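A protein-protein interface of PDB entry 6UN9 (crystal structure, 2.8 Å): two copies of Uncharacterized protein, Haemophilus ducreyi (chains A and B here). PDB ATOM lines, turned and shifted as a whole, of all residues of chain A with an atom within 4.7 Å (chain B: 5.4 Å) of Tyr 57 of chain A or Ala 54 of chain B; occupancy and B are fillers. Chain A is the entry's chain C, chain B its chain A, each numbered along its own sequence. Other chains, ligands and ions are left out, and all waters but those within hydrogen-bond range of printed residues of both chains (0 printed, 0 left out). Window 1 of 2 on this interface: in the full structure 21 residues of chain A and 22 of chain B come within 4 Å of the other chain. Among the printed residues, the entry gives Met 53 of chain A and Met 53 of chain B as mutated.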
ATOM      1  N   MET A  53      26.523  -5.811 -27.411  1.00  0.00           N
ATOM      2  CA  MET A  53      25.116  -5.907 -27.060  1.00  0.00           C
ATOM      3  C   MET A  53      24.394  -4.628 -27.386  1.00  0.00           C
ATOM      4  O   MET A  53      23.341  -4.637 -28.022  1.00  0.00           O
ATOM      5  CB  MET A  53      24.952  -6.187 -25.581  1.00  0.00           C
ATOM      6  CG  MET A  53      25.568  -7.463 -25.098  1.00  0.00           C
ATOM      7  SD  MET A  53      24.649  -7.878 -23.464  1.00  0.00           S
ATOM      8  CE  MET A  53      24.486  -6.050 -22.789  1.00  0.00           C
ATOM      9  N   ALA A  54      24.986  -3.519 -26.937  1.00  0.00           N
ATOM     10  CA  ALA A  54      24.424  -2.204 -27.221  1.00  0.00           C
ATOM     11  C   ALA A  54      24.071  -2.038 -28.699  1.00  0.00           C
ATOM     12  O   ALA A  54      23.048  -1.435 -29.034  1.00  0.00           O
ATOM     13  CB  ALA A  54      25.409  -1.119 -26.796  1.00  0.00           C
ATOM     14  N   GLU A  55      24.909  -2.561 -29.597  1.00  0.00           N
ATOM     15  CA  GLU A  55      24.736  -2.292 -31.019  1.00  0.00           C
ATOM     16  C   GLU A  55      23.780  -3.285 -31.668  1.00  0.00           C
ATOM     17  O   GLU A  55      23.092  -2.947 -32.643  1.00  0.00           O
ATOM     18  CB  GLU A  55      26.096  -2.301 -31.719  1.00  0.00           C
ATOM     19  CG  GLU A  55      26.742  -0.912 -31.776  1.00  0.00           C
ATOM     20  CD  GLU A  55      27.351  -0.599 -33.136  1.00  0.00           C
ATOM     21  OE1 GLU A  55      28.597  -0.512 -33.225  1.00  0.00           O
ATOM     22  OE2 GLU A  55      26.579  -0.444 -34.117  1.00  0.00           O
ATOM     23  N   ASP A  56      23.731  -4.506 -31.140  1.00  0.00           N
ATOM     24  CA  ASP A  56      22.641  -5.402 -31.487  1.00  0.00           C
ATOM     25  C   ASP A  56      21.296  -4.780 -31.145  1.00  0.00           C
ATOM     26  O   ASP A  56      20.360  -4.844 -31.948  1.00  0.00           O
ATOM     27  CB  ASP A  56      22.822  -6.733 -30.775  1.00  0.00           C
ATOM     28  CG  ASP A  56      24.083  -7.438 -31.202  1.00  0.00           C
ATOM     29  OD1 ASP A  56      24.821  -6.862 -32.031  1.00  0.00           O
ATOM     30  OD2 ASP A  56      24.317  -8.571 -30.730  1.00  0.00           O
ATOM     31  N   TYR A  57      21.186  -4.151 -29.971  1.00  0.00           N
ATOM     32  CA  TYR A  57      19.936  -3.518 -29.585  1.00  0.00           C
ATOM     33  C   TYR A  57      19.469  -2.519 -30.638  1.00  0.00           C
ATOM     34  O   TYR A  57      18.397  -2.711 -31.216  1.00  0.00           O
ATOM     35  CB  TYR A  57      20.037  -2.820 -28.236  1.00  0.00           C
ATOM     36  CG  TYR A  57      18.751  -2.138 -27.851  1.00  0.00           C
ATOM     37  CD1 TYR A  57      17.791  -2.815 -27.125  1.00  0.00           C
ATOM     38  CD2 TYR A  57      18.484  -0.831 -28.233  1.00  0.00           C
ATOM     39  CE1 TYR A  57      16.607  -2.215 -26.771  1.00  0.00           C
ATOM     40  CE2 TYR A  57      17.307  -0.211 -27.882  1.00  0.00           C
ATOM     41  CZ  TYR A  57      16.364  -0.908 -27.149  1.00  0.00           C
ATOM     42  OH  TYR A  57      15.170  -0.310 -26.797  1.00  0.00           O
ATOM     43  N   LYS A  58      20.229  -1.458 -30.920  1.00  0.00           N
ATOM     44  CA  LYS A  58      19.604  -0.491 -31.822  1.00  0.00           C
ATOM     45  C   LYS A  58      19.506  -1.001 -33.261  1.00  0.00           C
ATOM     46  O   LYS A  58      18.845  -0.359 -34.085  1.00  0.00           O
ATOM     47  CB  LYS A  58      20.317   0.867 -31.772  1.00  0.00           C
ATOM     48  CG  LYS A  58      19.360   2.017 -32.151  1.00  0.00           C
ATOM     49  CD  LYS A  58      19.841   3.391 -31.701  1.00  0.00           C
ATOM     50  CE  LYS A  58      19.683   4.424 -32.814  1.00  0.00           C
ATOM     51  NZ  LYS A  58      18.300   4.522 -33.329  1.00  0.00           N
ATOM     52  N   LYS A  59      20.109  -2.151 -33.572  1.00  0.00           N
ATOM     53  CA  LYS A  59      19.798  -2.878 -34.797  1.00  0.00           C
ATOM     54  C   LYS A  59      18.410  -3.516 -34.702  1.00  0.00           C
ATOM     55  O   LYS A  59      17.482  -3.115 -35.416  1.00  0.00           O
ATOM     56  CB  LYS A  59      20.880  -3.932 -35.074  1.00  0.00           C
ATOM     57  CG  LYS A  59      21.722  -3.632 -36.296  1.00  0.00           C
ATOM     58  CD  LYS A  59      21.919  -2.128 -36.469  1.00  0.00           C
ATOM     59  CE  LYS A  59      22.631  -1.784 -37.779  1.00  0.00           C
ATOM     60  NZ  LYS A  59      23.381  -0.486 -37.670  1.00  0.00           N
ATOM     61  N   LEU A  60      18.267  -4.495 -33.802  1.00  0.00           N
ATOM     62  CA  LEU A  60      16.969  -5.056 -33.450  1.00  0.00           C
ATOM     63  C   LEU A  60      15.952  -4.002 -33.019  1.00  0.00           C
ATOM     64  O   LEU A  60      14.753  -4.286 -32.987  1.00  0.00           O
ATOM     65  CB  LEU A  60      17.150  -6.087 -32.328  1.00  0.00           C
ATOM     66  CG  LEU A  60      15.927  -6.917 -31.940  1.00  0.00           C
ATOM     67  CD1 LEU A  60      15.613  -7.892 -33.062  1.00  0.00           C
ATOM     68  CD2 LEU A  60      16.097  -7.646 -30.626  1.00  0.00           C
ATOM     69  N   TYR A  61      16.379  -2.797 -32.664  1.00  0.00           N
ATOM     70  CA  TYR A  61      15.360  -1.799 -32.386  1.00  0.00           C
ATOM     71  C   TYR A  61      14.818  -1.203 -33.673  1.00  0.00           C
ATOM     72  O   TYR A  61      13.605  -1.114 -33.848  1.00  0.00           O
ATOM     73  CB  TYR A  61      15.894  -0.695 -31.480  1.00  0.00           C
ATOM     74  CG  TYR A  61      14.982   0.516 -31.435  1.00  0.00           C
ATOM     75  CD1 TYR A  61      14.021   0.652 -30.445  1.00  0.00           C
ATOM     76  CD2 TYR A  61      15.093   1.530 -32.381  1.00  0.00           C
ATOM     77  CE1 TYR A  61      13.199   1.762 -30.398  1.00  0.00           C
ATOM     78  CE2 TYR A  61      14.277   2.625 -32.351  1.00  0.00           C
ATOM     79  CZ  TYR A  61      13.335   2.745 -31.355  1.00  0.00           C
ATOM     80  OH  TYR A  61      12.534   3.861 -31.332  1.00  0.00           O
ATOM     81  N   PHE A  80       7.062   4.321 -28.752  1.00  0.00           N
ATOM     82  CA  PHE A  80       8.447   3.875 -28.619  1.00  0.00           C
ATOM     83  C   PHE A  80       9.250   4.126 -29.887  1.00  0.00           C
ATOM     84  O   PHE A  80      10.452   4.412 -29.822  1.00  0.00           O
ATOM     85  CB  PHE A  80       8.479   2.392 -28.259  1.00  0.00           C
ATOM     86  CG  PHE A  80       9.831   1.907 -27.820  1.00  0.00           C
ATOM     87  CD1 PHE A  80      10.604   2.666 -26.964  1.00  0.00           C
ATOM     88  CD2 PHE A  80      10.320   0.684 -28.252  1.00  0.00           C
ATOM     89  CE1 PHE A  80      11.833   2.224 -26.561  1.00  0.00           C
ATOM     90  CE2 PHE A  80      11.548   0.234 -27.844  1.00  0.00           C
ATOM     91  CZ  PHE A  80      12.305   1.003 -27.000  1.00  0.00           C
ATOM     92  N   LEU B  50      11.151  -4.534 -25.522  1.00  0.00           N
ATOM     93  CA  LEU B  50      12.424  -4.017 -26.011  1.00  0.00           C
ATOM     94  C   LEU B  50      12.936  -2.878 -25.144  1.00  0.00           C
ATOM     95  O   LEU B  50      14.148  -2.733 -24.966  1.00  0.00           O
ATOM     96  CB  LEU B  50      12.301  -3.537 -27.456  1.00  0.00           C
ATOM     97  CG  LEU B  50      12.468  -4.611 -28.518  1.00  0.00           C
ATOM     98  CD1 LEU B  50      12.157  -4.055 -29.918  1.00  0.00           C
ATOM     99  CD2 LEU B  50      13.856  -5.170 -28.449  1.00  0.00           C
ATOM    100  N   GLU B  51      12.035  -2.045 -24.624  1.00  0.00           N
ATOM    101  CA  GLU B  51      12.472  -0.990 -23.725  1.00  0.00           C
ATOM    102  C   GLU B  51      12.917  -1.571 -22.390  1.00  0.00           C
ATOM    103  O   GLU B  51      13.947  -1.158 -21.845  1.00  0.00           O
ATOM    104  CB  GLU B  51      11.365   0.044 -23.534  1.00  0.00           C
ATOM    105  CG  GLU B  51      11.908   1.406 -23.136  1.00  0.00           C
ATOM    106  CD  GLU B  51      10.823   2.410 -22.813  1.00  0.00           C
ATOM    107  OE1 GLU B  51      11.154   3.615 -22.716  1.00  0.00           O
ATOM    108  OE2 GLU B  51       9.649   1.998 -22.652  1.00  0.00           O
ATOM    109  N   ASN B  52      12.144  -2.515 -21.846  1.00  0.00           N
ATOM    110  CA  ASN B  52      12.656  -3.433 -20.838  1.00  0.00           C
ATOM    111  C   ASN B  52      14.119  -3.811 -21.075  1.00  0.00           C
ATOM    112  O   ASN B  52      14.963  -3.662 -20.187  1.00  0.00           O
ATOM    113  CB  ASN B  52      11.795  -4.692 -20.824  1.00  0.00           C
ATOM    114  CG  ASN B  52      10.559  -4.512 -20.020  1.00  0.00           C
ATOM    115  OD1 ASN B  52      10.213  -3.384 -19.674  1.00  0.00           O
ATOM    116  ND2 ASN B  52       9.877  -5.613 -19.699  1.00  0.00           N
ATOM    117  N   MET B  53      14.431  -4.314 -22.266  1.00  0.00           N
ATOM    118  CA  MET B  53      15.797  -4.703 -22.606  1.00  0.00           C
ATOM    119  C   MET B  53      16.785  -3.551 -22.492  1.00  0.00           C
ATOM    120  O   MET B  53      17.931  -3.754 -22.118  1.00  0.00           O
ATOM    121  CB  MET B  53      15.854  -5.260 -24.030  1.00  0.00           C
ATOM    122  CG  MET B  53      15.549  -6.732 -24.137  1.00  0.00           C
ATOM    123  SD  MET B  53      17.109  -7.724 -24.737  1.00  0.00           S
ATOM    124  CE  MET B  53      18.273  -7.442 -23.187  1.00  0.00           C
ATOM    125  N   ALA B  54      16.320  -2.354 -22.857  1.00  0.00           N
ATOM    126  CA  ALA B  54      17.143  -1.151 -22.834  1.00  0.00           C
ATOM    127  C   ALA B  54      17.361  -0.639 -21.412  1.00  0.00           C
ATOM    128  O   ALA B  54      18.493  -0.329 -21.025  1.00  0.00           O
ATOM    129  CB  ALA B  54      16.497  -0.062 -23.688  1.00  0.00           C
ATOM    130  N   GLU B  55      16.291  -0.526 -20.629  1.00  0.00           N
ATOM    131  CA  GLU B  55      16.447  -0.080 -19.262  1.00  0.00           C
ATOM    132  C   GLU B  55      17.195  -1.089 -18.395  1.00  0.00           C
ATOM    133  O   GLU B  55      17.571  -0.751 -17.269  1.00  0.00           O
ATOM    134  CB  GLU B  55      15.080   0.197 -18.651  1.00  0.00           C
ATOM    135  CG  GLU B  55      14.438  -1.052 -18.094  1.00  0.00           C
ATOM    136  CD  GLU B  55      13.306  -0.739 -17.141  1.00  0.00           C
ATOM    137  OE1 GLU B  55      12.503  -1.658 -16.844  1.00  0.00           O
ATOM    138  OE2 GLU B  55      13.219   0.427 -16.697  1.00  0.00           O
ATOM    139  N   ASP B  56      17.401  -2.317 -18.864  1.00  0.00           N
ATOM    140  CA  ASP B  56      18.225  -3.257 -18.119  1.00  0.00           C
ATOM    141  C   ASP B  56      19.671  -3.206 -18.557  1.00  0.00           C
ATOM    142  O   ASP B  56      20.568  -3.440 -17.736  1.00  0.00           O
ATOM    143  CB  ASP B  56      17.690  -4.683 -18.259  1.00  0.00           C
ATOM    144  CG  ASP B  56      16.600  -4.976 -17.259  1.00  0.00           C
ATOM    145  OD1 ASP B  56      16.156  -4.016 -16.595  1.00  0.00           O
ATOM    146  OD2 ASP B  56      16.190  -6.147 -17.116  1.00  0.00           O
ATOM    147  N   TYR B  57      19.898  -2.913 -19.834  1.00  0.00           N
ATOM    148  CA  TYR B  57      21.221  -2.514 -20.284  1.00  0.00           C
ATOM    149  C   TYR B  57      21.723  -1.305 -19.498  1.00  0.00           C
ATOM    150  O   TYR B  57      22.812  -1.336 -18.915  1.00  0.00           O
ATOM    151  CB  TYR B  57      21.184  -2.213 -21.776  1.00  0.00           C
ATOM    152  CG  TYR B  57      22.508  -1.759 -22.294  1.00  0.00           C
ATOM    153  CD1 TYR B  57      23.520  -2.674 -22.534  1.00  0.00           C
ATOM    154  CD2 TYR B  57      22.762  -0.415 -22.533  1.00  0.00           C
ATOM    155  CE1 TYR B  57      24.759  -2.266 -23.008  1.00  0.00           C
ATOM    156  CE2 TYR B  57      23.996   0.009 -23.008  1.00  0.00           C
ATOM    157  CZ  TYR B  57      24.995  -0.920 -23.246  1.00  0.00           C
ATOM    158  OH  TYR B  57      26.236  -0.513 -23.720  1.00  0.00           O
ATOM    159  N   LYS B  58      20.932  -0.228 -19.460  1.00  0.00           N
ATOM    160  CA  LYS B  58      21.341   0.970 -18.743  1.00  0.00           C
ATOM    161  C   LYS B  58      21.543   0.714 -17.254  1.00  0.00           C
ATOM    162  O   LYS B  58      22.177   1.524 -16.570  1.00  0.00           O
ATOM    163  CB  LYS B  58      20.321   2.085 -18.962  1.00  0.00           C
ATOM    164  CG  LYS B  58      20.871   3.235 -19.801  1.00  0.00           C
ATOM    165  CD  LYS B  58      19.869   4.388 -19.939  1.00  0.00           C
ATOM    166  CE  LYS B  58      20.571   5.762 -19.956  1.00  0.00           C
ATOM    167  NZ  LYS B  58      19.710   6.892 -20.442  1.00  0.00           N
ATOM    168  N   LYS B  59      21.015  -0.388 -16.732  1.00  0.00           N
ATOM    169  CA  LYS B  59      21.441  -0.840 -15.417  1.00  0.00           C
ATOM    170  C   LYS B  59      22.839  -1.444 -15.491  1.00  0.00           C
ATOM    171  O   LYS B  59      23.775  -0.962 -14.845  1.00  0.00           O
ATOM    172  CB  LYS B  59      20.433  -1.846 -14.864  1.00  0.00           C
ATOM    173  CG  LYS B  59      19.261  -1.219 -14.104  1.00  0.00           C
ATOM    174  CD  LYS B  59      18.539  -2.274 -13.276  1.00  0.00           C
ATOM    175  CE  LYS B  59      17.581  -1.662 -12.255  1.00  0.00           C
ATOM    176  NZ  LYS B  59      16.256  -1.274 -12.863  1.00  0.00           N
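Met 53 of chain A touches Tyr 57 of chain B, but with the chains exchanged Tyr 57 of chain A does not touch Met 53 of chain B (4.2 Å).
Ala 54 of chain A touches Tyr 57 of chain B, and with the chains exchanged Tyr 57 of chain A touches Ala 54 of chain B.
Positions printed for both chains: 53, 54, 55, 56, 57, 58 and 59.
Of the 7 pairs that touch across the chains among the printed residues, 2 have their exchanged pair printed and touching as well.
Tyr 57 of chain A touches just these residues of chain B: Leu 50 (3.1 Å) and Ala 54 (3.4 Å).
Of chain A, only Tyr 57 (3.4 Å) comes within 4 Å of Ala 54 of chain B.
Of the printed residues of chain A, Glu 51 of chain B touches Phe 80 (3.5 Å).
Of the printed residues of chain A, Tyr 57 of chain B touches Met 53 (3.5 Å) and Ala 54 (3.2 Å).
Of the printed residues of chain B, Ala 54 of chain A touches Tyr 57 (3.2 Å).
Of the printed residues of chain B, Phe 80 of chain A touches Leu 50 (3.9 Å) and Glu 51 (3.5 Å).
Of the printed residues of chain B, Leu 60 of chain A touches Leu 50 (3.99 Å).
Lys 59 of chain B touches none of the printed residues of chain A.
The nearest printed residue of chain A that does not touch Ala 54 of chain B is Phe 80 of chain A (5.4 Å).
The nearest printed residue of chain A that does not touch Leu 50 of chain B is Tyr 61 of chain A (4.6 Å).
O of Phe 80 of chain A is in hydrogen-bond range of OH of Tyr 61 of chain A (2.6 Å).
CE of Met 53 of chain A touches CD1 of Tyr 57 of chain B (3.5 Å).
OH of Tyr 57 of chain B touches CB of Ala 54 of chain A (3.2 Å).
Tyr 57 of chain A touches Ala 54 of chain B (OH to CB, 3.4 Å).
Leu 60 of chain A touches Leu 50 of chain B (CD2 to CD2, 3.99 Å).
Leu 50 of chain B touches Phe 80 of chain A (CB to CE2, 3.9 Å).
Phe 80 of chain A touches Glu 51 of chain B (CE1 to CG, 3.5 Å).
The backbone carbonyl oxygen (O) of Leu 50 of chain B sits close to the side-chain hydroxyl (OH) of Tyr 57 of chain A (3.2 Å).
Printed residues of chain A that touch a printed residue of chain B: Met 53, Ala 54, Tyr 57, Leu 60 and Phe 80.
Hydrophobic or aromatic side chains of chain A within 4 Å of the printed part of chain B: Met 53, Ala 54, Tyr 57, Leu 60 and Phe 80.
Among the printed residues, 7 pairs touch across the chains.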
